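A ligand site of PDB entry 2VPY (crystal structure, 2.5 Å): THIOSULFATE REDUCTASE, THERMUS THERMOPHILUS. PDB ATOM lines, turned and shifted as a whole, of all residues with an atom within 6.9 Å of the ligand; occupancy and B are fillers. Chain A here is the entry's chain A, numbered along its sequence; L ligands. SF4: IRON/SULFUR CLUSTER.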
ATOM      1  N   ILE A  43      13.429 -10.921  -1.180  1.00  0.00           N
ATOM      2  CA  ILE A  43      12.482 -11.466  -0.206  1.00  0.00           C
ATOM      3  C   ILE A  43      11.439 -12.373  -0.889  1.00  0.00           C
ATOM      4  O   ILE A  43      11.064 -12.139  -2.036  1.00  0.00           O
ATOM      5  CB  ILE A  43      11.669 -10.318   0.451  1.00  0.00           C
ATOM      6  CG1 ILE A  43      12.582  -9.109   0.663  1.00  0.00           C
ATOM      7  CG2 ILE A  43      11.042 -10.773   1.761  1.00  0.00           C
ATOM      8  CD1 ILE A  43      12.284  -8.298   1.929  1.00  0.00           C
ATOM      9  N   CYS A  44      10.996 -13.432  -0.206  1.00  0.00           N
ATOM     10  CA  CYS A  44       9.973 -14.307  -0.785  1.00  0.00           C
ATOM     11  C   CYS A  44       8.579 -13.726  -0.450  1.00  0.00           C
ATOM     12  O   CYS A  44       8.332 -13.369   0.710  1.00  0.00           O
ATOM     13  CB  CYS A  44      10.084 -15.746  -0.231  1.00  0.00           C
ATOM     14  SG  CYS A  44       8.622 -16.775  -0.573  1.00  0.00           S
ATOM     15  N   GLU A  45       7.688 -13.579  -1.430  1.00  0.00           N
ATOM     16  CA  GLU A  45       6.329 -13.110  -1.132  1.00  0.00           C
ATOM     17  C   GLU A  45       5.389 -14.352  -1.127  1.00  0.00           C
ATOM     18  O   GLU A  45       4.151 -14.234  -1.138  1.00  0.00           O
ATOM     19  CB  GLU A  45       5.841 -12.019  -2.135  1.00  0.00           C
ATOM     20  CG  GLU A  45       4.635 -11.137  -1.641  1.00  0.00           C
ATOM     21  CD  GLU A  45       4.877 -10.375  -0.336  1.00  0.00           C
ATOM     22  OE1 GLU A  45       6.039  -9.948  -0.082  1.00  0.00           O
ATOM     23  OE2 GLU A  45       3.902 -10.157   0.433  1.00  0.00           O
ATOM     24  N   GLY A  46       6.006 -15.531  -1.078  1.00  0.00           N
ATOM     25  CA  GLY A  46       5.293 -16.801  -1.012  1.00  0.00           C
ATOM     26  C   GLY A  46       4.228 -16.805   0.097  1.00  0.00           C
ATOM     27  O   GLY A  46       3.148 -17.376  -0.065  1.00  0.00           O
ATOM     28  N   CYS A  47       4.541 -16.192   1.231  1.00  0.00           N
ATOM     29  CA  CYS A  47       3.618 -16.046   2.352  1.00  0.00           C
ATOM     30  C   CYS A  47       4.174 -14.903   3.226  1.00  0.00           C
ATOM     31  O   CYS A  47       5.132 -14.230   2.838  1.00  0.00           O
ATOM     32  CB  CYS A  47       3.454 -17.343   3.181  1.00  0.00           C
ATOM     33  SG  CYS A  47       4.803 -17.759   4.335  1.00  0.00           S
ATOM     34  N   PHE A  48       3.605 -14.684   4.395  1.00  0.00           N
ATOM     35  CA  PHE A  48       4.063 -13.575   5.182  1.00  0.00           C
ATOM     36  C   PHE A  48       5.299 -13.780   6.048  1.00  0.00           C
ATOM     37  O   PHE A  48       5.740 -12.870   6.729  1.00  0.00           O
ATOM     38  CB  PHE A  48       2.845 -13.052   5.989  1.00  0.00           C
ATOM     39  CG  PHE A  48       1.563 -12.928   5.145  1.00  0.00           C
ATOM     40  CD1 PHE A  48       0.331 -13.369   5.621  1.00  0.00           C
ATOM     41  CD2 PHE A  48       1.630 -12.423   3.841  1.00  0.00           C
ATOM     42  CE1 PHE A  48      -0.822 -13.301   4.800  1.00  0.00           C
ATOM     43  CE2 PHE A  48       0.476 -12.345   3.018  1.00  0.00           C
ATOM     44  CZ  PHE A  48      -0.736 -12.785   3.490  1.00  0.00           C
ATOM     45  N   TRP A  49       5.906 -14.958   5.993  1.00  0.00           N
ATOM     46  CA  TRP A  49       7.111 -15.184   6.798  1.00  0.00           C
ATOM     47  C   TRP A  49       8.257 -14.285   6.305  1.00  0.00           C
ATOM     48  O   TRP A  49       9.165 -13.953   7.061  1.00  0.00           O
ATOM     49  CB  TRP A  49       7.492 -16.657   6.758  1.00  0.00           C
ATOM     50  CG  TRP A  49       8.379 -17.117   7.887  1.00  0.00           C
ATOM     51  CD1 TRP A  49       9.673 -17.524   7.784  1.00  0.00           C
ATOM     52  CD2 TRP A  49       8.014 -17.301   9.266  1.00  0.00           C
ATOM     53  NE1 TRP A  49      10.138 -17.949   9.004  1.00  0.00           N
ATOM     54  CE2 TRP A  49       9.146 -17.823   9.931  1.00  0.00           C
ATOM     55  CE3 TRP A  49       6.838 -17.079   9.998  1.00  0.00           C
ATOM     56  CZ2 TRP A  49       9.150 -18.115  11.305  1.00  0.00           C
ATOM     57  CZ3 TRP A  49       6.834 -17.368  11.383  1.00  0.00           C
ATOM     58  CH2 TRP A  49       7.989 -17.879  12.008  1.00  0.00           C
ATOM     59  N   ARG A  50       8.170 -13.941   5.027  1.00  0.00           N
ATOM     60  CA  ARG A  50       9.105 -13.100   4.284  1.00  0.00           C
ATOM     61  C   ARG A  50      10.599 -13.532   4.364  1.00  0.00           C
ATOM     62  O   ARG A  50      11.468 -12.744   4.723  1.00  0.00           O
ATOM     63  CB  ARG A  50       8.881 -11.627   4.708  1.00  0.00           C
ATOM     64  CG  ARG A  50       7.438 -11.075   4.381  1.00  0.00           C
ATOM     65  CD  ARG A  50       7.126  -9.676   4.972  1.00  0.00           C
ATOM     66  NE  ARG A  50       6.114  -9.700   6.034  1.00  0.00           N
ATOM     67  CZ  ARG A  50       4.826  -9.348   5.907  1.00  0.00           C
ATOM     68  NH1 ARG A  50       4.343  -8.916   4.753  1.00  0.00           N
ATOM     69  NH2 ARG A  50       3.996  -9.445   6.956  1.00  0.00           N
ATOM     70  N   CYS A  51      10.889 -14.787   3.988  1.00  0.00           N
ATOM     71  CA  CYS A  51      12.260 -15.298   4.009  1.00  0.00           C
ATOM     72  C   CYS A  51      13.135 -14.528   3.002  1.00  0.00           C
ATOM     73  O   CYS A  51      12.651 -14.100   1.944  1.00  0.00           O
ATOM     74  CB  CYS A  51      12.307 -16.814   3.664  1.00  0.00           C
ATOM     75  SG  CYS A  51      11.188 -17.853   4.640  1.00  0.00           S
ATOM     76  N   GLY A  52      14.408 -14.351   3.373  1.00  0.00           N
ATOM     77  CA  GLY A  52      15.389 -13.702   2.531  1.00  0.00           C
ATOM     78  C   GLY A  52      15.850 -14.774   1.547  1.00  0.00           C
ATOM     79  O   GLY A  52      16.180 -15.904   1.955  1.00  0.00           O
ATOM     80  N   ILE A  53      15.874 -14.422   0.267  1.00  0.00           N
ATOM     81  CA  ILE A  53      16.253 -15.337  -0.803  1.00  0.00           C
ATOM     82  C   ILE A  53      17.148 -14.710  -1.877  1.00  0.00           C
ATOM     83  O   ILE A  53      17.244 -13.490  -1.979  1.00  0.00           O
ATOM     84  CB  ILE A  53      14.985 -15.884  -1.552  1.00  0.00           C
ATOM     85  CG1 ILE A  53      14.133 -14.733  -2.068  1.00  0.00           C
ATOM     86  CG2 ILE A  53      14.138 -16.781  -0.628  1.00  0.00           C
ATOM     87  CD1 ILE A  53      13.305 -15.007  -3.293  1.00  0.00           C
ATOM     88  N   LYS A  73      16.188 -16.046   8.617  1.00  0.00           N
ATOM     89  CA  LYS A  73      14.949 -16.757   8.305  1.00  0.00           C
ATOM     90  C   LYS A  73      15.179 -17.985   7.423  1.00  0.00           C
ATOM     91  O   LYS A  73      14.835 -19.096   7.826  1.00  0.00           O
ATOM     92  CB  LYS A  73      13.940 -15.818   7.639  1.00  0.00           C
ATOM     93  CG  LYS A  73      13.318 -14.813   8.578  1.00  0.00           C
ATOM     94  CD  LYS A  73      12.070 -14.215   7.956  1.00  0.00           C
ATOM     95  CE  LYS A  73      11.244 -13.425   8.968  1.00  0.00           C
ATOM     96  NZ  LYS A  73      10.227 -14.287   9.659  1.00  0.00           N
ATOM     97  N   SER A  74      15.790 -17.814   6.255  1.00  0.00           N
ATOM     98  CA  SER A  74      16.050 -18.993   5.427  1.00  0.00           C
ATOM     99  C   SER A  74      17.278 -19.814   5.824  1.00  0.00           C
ATOM    100  O   SER A  74      17.216 -21.037   5.836  1.00  0.00           O
ATOM    101  CB  SER A  74      16.126 -18.598   3.953  1.00  0.00           C
ATOM    102  OG  SER A  74      16.896 -17.437   3.750  1.00  0.00           O
ATOM    103  N   ARG A  77      18.082 -22.652   3.440  1.00  0.00           N
ATOM    104  CA  ARG A  77      16.935 -23.479   3.061  1.00  0.00           C
ATOM    105  C   ARG A  77      15.718 -22.673   2.571  1.00  0.00           C
ATOM    106  O   ARG A  77      15.684 -21.441   2.692  1.00  0.00           O
ATOM    107  CB  ARG A  77      16.469 -24.384   4.212  1.00  0.00           C
ATOM    108  CG  ARG A  77      17.465 -24.670   5.298  1.00  0.00           C
ATOM    109  CD  ARG A  77      18.355 -25.814   4.923  1.00  0.00           C
ATOM    110  NE  ARG A  77      19.597 -25.365   4.294  1.00  0.00           N
ATOM    111  CZ  ARG A  77      20.785 -25.424   4.882  1.00  0.00           C
ATOM    112  NH1 ARG A  77      20.874 -25.921   6.099  1.00  0.00           N
ATOM    113  NH2 ARG A  77      21.878 -25.003   4.268  1.00  0.00           N
ATOM    114  N   LEU A  78      14.717 -23.389   2.067  1.00  0.00           N
ATOM    115  CA  LEU A  78      13.478 -22.836   1.540  1.00  0.00           C
ATOM    116  C   LEU A  78      12.389 -23.937   1.531  1.00  0.00           C
ATOM    117  O   LEU A  78      12.670 -25.107   1.270  1.00  0.00           O
ATOM    118  CB  LEU A  78      13.703 -22.323   0.109  1.00  0.00           C
ATOM    119  CG  LEU A  78      13.233 -20.914  -0.304  1.00  0.00           C
ATOM    120  CD1 LEU A  78      13.671 -19.890   0.735  1.00  0.00           C
ATOM    121  CD2 LEU A  78      13.776 -20.562  -1.694  1.00  0.00           C
ATOM    122  N   CYS A  79      11.147 -23.549   1.842  1.00  0.00           N
ATOM    123  CA  CYS A  79      10.036 -24.484   1.840  1.00  0.00           C
ATOM    124  C   CYS A  79       9.556 -24.598   0.383  1.00  0.00           C
ATOM    125  O   CYS A  79       9.957 -23.827  -0.491  1.00  0.00           O
ATOM    126  CB  CYS A  79       8.877 -23.982   2.738  1.00  0.00           C
ATOM    127  SG  CYS A  79       7.656 -22.781   1.958  1.00  0.00           S
ATOM    128  N   PRO A  80       8.646 -25.564   0.107  1.00  0.00           N
ATOM    129  CA  PRO A  80       8.106 -25.791  -1.251  1.00  0.00           C
ATOM    130  C   PRO A  80       7.464 -24.553  -1.886  1.00  0.00           C
ATOM    131  O   PRO A  80       7.659 -24.255  -3.077  1.00  0.00           O
ATOM    132  CB  PRO A  80       7.138 -26.954  -1.073  1.00  0.00           C
ATOM    133  CG  PRO A  80       6.765 -26.904   0.397  1.00  0.00           C
ATOM    134  CD  PRO A  80       8.016 -26.444   1.101  1.00  0.00           C
ATOM    135  N   ARG A  81       6.684 -23.827  -1.108  1.00  0.00           N
ATOM    136  CA  ARG A  81       6.003 -22.618  -1.579  1.00  0.00           C
ATOM    137  C   ARG A  81       6.995 -21.547  -2.009  1.00  0.00           C
ATOM    138  O   ARG A  81       6.733 -20.803  -2.940  1.00  0.00           O
ATOM    139  CB  ARG A  81       5.055 -22.108  -0.490  1.00  0.00           C
ATOM    140  CG  ARG A  81       3.895 -23.057  -0.277  1.00  0.00           C
ATOM    141  CD  ARG A  81       3.119 -22.814   1.030  1.00  0.00           C
ATOM    142  NE  ARG A  81       3.974 -22.770   2.213  1.00  0.00           N
ATOM    143  CZ  ARG A  81       4.145 -21.696   2.991  1.00  0.00           C
ATOM    144  NH1 ARG A  81       3.533 -20.553   2.708  1.00  0.00           N
ATOM    145  NH2 ARG A  81       4.967 -21.765   4.045  1.00  0.00           N
ATOM    146  N   GLY A  82       8.138 -21.468  -1.328  1.00  0.00           N
ATOM    147  CA  GLY A  82       9.151 -20.504  -1.666  1.00  0.00           C
ATOM    148  C   GLY A  82       9.785 -20.866  -2.984  1.00  0.00           C
ATOM    149  O   GLY A  82      10.024 -20.009  -3.843  1.00  0.00           O
ATOM    150  N   GLN A  83      10.020 -22.165  -3.176  1.00  0.00           N
ATOM    151  CA  GLN A  83      10.634 -22.660  -4.408  1.00  0.00           C
ATOM    152  C   GLN A  83       9.742 -22.494  -5.647  1.00  0.00           C
ATOM    153  O   GLN A  83      10.222 -22.154  -6.735  1.00  0.00           O
ATOM    154  CB  GLN A  83      11.047 -24.149  -4.289  1.00  0.00           C
ATOM    155  CG  GLN A  83      12.142 -24.468  -3.275  1.00  0.00           C
ATOM    156  CD  GLN A  83      13.550 -24.139  -3.751  1.00  0.00           C
ATOM    157  OE1 GLN A  83      14.524 -24.299  -3.018  1.00  0.00           O
ATOM    158  NE2 GLN A  83      13.660 -23.685  -4.994  1.00  0.00           N
ATOM    159  N   ALA A  85       7.031 -20.356  -5.811  1.00  0.00           N
ATOM    160  CA  ALA A  85       6.489 -18.998  -5.875  1.00  0.00           C
ATOM    161  C   ALA A  85       6.751 -18.193  -7.137  1.00  0.00           C
ATOM    162  O   ALA A  85       5.914 -17.402  -7.568  1.00  0.00           O
ATOM    163  CB  ALA A  85       6.923 -18.184  -4.622  1.00  0.00           C
ATOM    164  N   THR A 214       3.985 -24.702   6.943  1.00  0.00           N
ATOM    165  CA  THR A 214       5.321 -24.888   6.510  1.00  0.00           C
ATOM    166  C   THR A 214       6.274 -23.683   6.514  1.00  0.00           C
ATOM    167  O   THR A 214       7.227 -23.597   5.721  1.00  0.00           O
ATOM    168  CB  THR A 214       5.193 -25.652   5.162  1.00  0.00           C
ATOM    169  OG1 THR A 214       6.078 -26.761   5.128  1.00  0.00           O
ATOM    170  CG2 THR A 214       5.366 -24.750   3.973  1.00  0.00           C
ATOM    171  N   HIS A 215       5.999 -22.749   7.440  1.00  0.00           N
ATOM    172  CA  HIS A 215       6.808 -21.546   7.696  1.00  0.00           C
ATOM    173  C   HIS A 215       8.229 -22.074   7.861  1.00  0.00           C
ATOM    174  O   HIS A 215       8.516 -22.889   8.755  1.00  0.00           O
ATOM    175  CB  HIS A 215       6.331 -20.807   8.975  1.00  0.00           C
ATOM    176  CG  HIS A 215       5.260 -19.805   8.727  1.00  0.00           C
ATOM    177  ND1 HIS A 215       4.426 -19.324   9.718  1.00  0.00           N
ATOM    178  CD2 HIS A 215       4.879 -19.214   7.590  1.00  0.00           C
ATOM    179  CE1 HIS A 215       3.568 -18.470   9.187  1.00  0.00           C
ATOM    180  NE2 HIS A 215       3.820 -18.396   7.894  1.00  0.00           N
ATOM    181  N   ASN A 216       9.073 -21.562   6.980  1.00  0.00           N
ATOM    182  CA  ASN A 216      10.456 -21.982   6.917  1.00  0.00           C
ATOM    183  C   ASN A 216      11.225 -22.262   8.194  1.00  0.00           C
ATOM    184  O   ASN A 216      11.431 -23.415   8.590  1.00  0.00           O
ATOM    185  CB  ASN A 216      11.262 -21.031   6.049  1.00  0.00           C
ATOM    186  CG  ASN A 216      12.558 -21.640   5.572  1.00  0.00           C
ATOM    187  OD1 ASN A 216      12.928 -22.720   6.031  1.00  0.00           O
ATOM    188  ND2 ASN A 216      13.238 -20.964   4.652  1.00  0.00           N
ATOM    189  N   THR A 217      11.647 -21.184   8.848  1.00  0.00           N
ATOM    190  CA  THR A 217      12.477 -21.264  10.042  1.00  0.00           C
ATOM    191  C   THR A 217      11.943 -22.109  11.166  1.00  0.00           C
ATOM    192  O   THR A 217      12.707 -22.799  11.856  1.00  0.00           O
ATOM    193  CB  THR A 217      12.818 -19.855  10.632  1.00  0.00           C
ATOM    194  OG1 THR A 217      12.836 -18.879   9.599  1.00  0.00           O
ATOM    195  CG2 THR A 217      14.184 -19.894  11.349  1.00  0.00           C
ATOM    196  N   THR A 630      -0.212 -21.992  -0.558  1.00  0.00           N
ATOM    197  CA  THR A 630      -0.386 -20.898   0.386  1.00  0.00           C
ATOM    198  C   THR A 630      -1.912 -20.531   0.343  1.00  0.00           C
ATOM    199  O   THR A 630      -2.485 -20.473  -0.744  1.00  0.00           O
ATOM    200  CB  THR A 630       0.497 -19.690  -0.012  1.00  0.00           C
ATOM    201  OG1 THR A 630       1.879 -20.019   0.131  1.00  0.00           O
ATOM    202  CG2 THR A 630       0.177 -18.489   0.874  1.00  0.00           C
HETATM  203 FE1  SF4 L   1       9.385 -18.340   3.412  1.00  0.00          FE
HETATM  204 FE2  SF4 L   1       8.110 -20.555   2.491  1.00  0.00          FE
HETATM  205 FE3  SF4 L   1       6.718 -18.311   3.127  1.00  0.00          FE
HETATM  206 FE4  SF4 L   1       8.276 -18.338   0.903  1.00  0.00          FE
HETATM  207  S1  SF4 L   1       6.429 -19.623   1.265  1.00  0.00           S
HETATM  208  S2  SF4 L   1       8.152 -16.664   2.469  1.00  0.00           S
HETATM  209  S3  SF4 L   1       9.994 -19.638   1.607  1.00  0.00           S
HETATM  210  S4  SF4 L   1       7.902 -19.622   4.585  1.00  0.00           S
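The guanidinium group (NH1) of Arg 81 sits close to a sulfur (S1) of the ligand, 3.4 Å away. FE4 of the ligand is bound by SG of Cys 44, 2.2 Å away. The backbone NH of Arg 50 lies close to a sulfur (S2) of the ligand, 3.7 Å away. N of Cys 51 lies close to S2 of the ligand. The backbone NH (N) of Gly 82 lies close to a sulfur (S1) of the ligand. FE1 of the ligand is bound by SG of Cys 51. SG of Cys 47 is bound to FE3 of the ligand, at 2.3 Å. The side-chain sulfur of Cys 79 binds an iron atom (FE2) of the ligand (2.3 Å). N of Asn 216 lies close to S4 of the ligand.
O of Trp 49 is in hydrogen-bond range of NZ of Lys 73 (2.8 Å). The side-chain sulfur of Cys 47 lies close to a ring nitrogen (NE2) of His 215, at 3.7 Å. SG of Cys 47 sits close to NH1 of Arg 81. OG1 of Thr 217 is in hydrogen-bond range of NE1 of Trp 49, 2.9 Å away. The guanidinium group of Arg 81 sits close to the backbone carbonyl oxygen of Thr 214 (3.4 Å). SG of Cys 47 lies close to N of Trp 49 (3.4 Å). The guanidinium group of Arg 81 is in hydrogen-bond range of the side-chain hydroxyl of Thr 630 (3.1 Å). The backbone carbonyl oxygen of Gly 46 lies within hydrogen-bond range of the side-chain hydroxyl of Thr 630, at 2.9 Å.
C of Gly 46 touches S1 of the ligand (3.8 Å). Trp 49 touches the ligand. CD1 of Leu 78 touches S3 of the ligand, 3.8 Å away. CA of His 215 touches S4 of the ligand (3.8 Å). Hydrophobic or aromatic side chains within 4 Å of the ligand: Trp 49 and Leu 78. Of the 26 residues printed, 12 come within 4 Å of the ligand.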
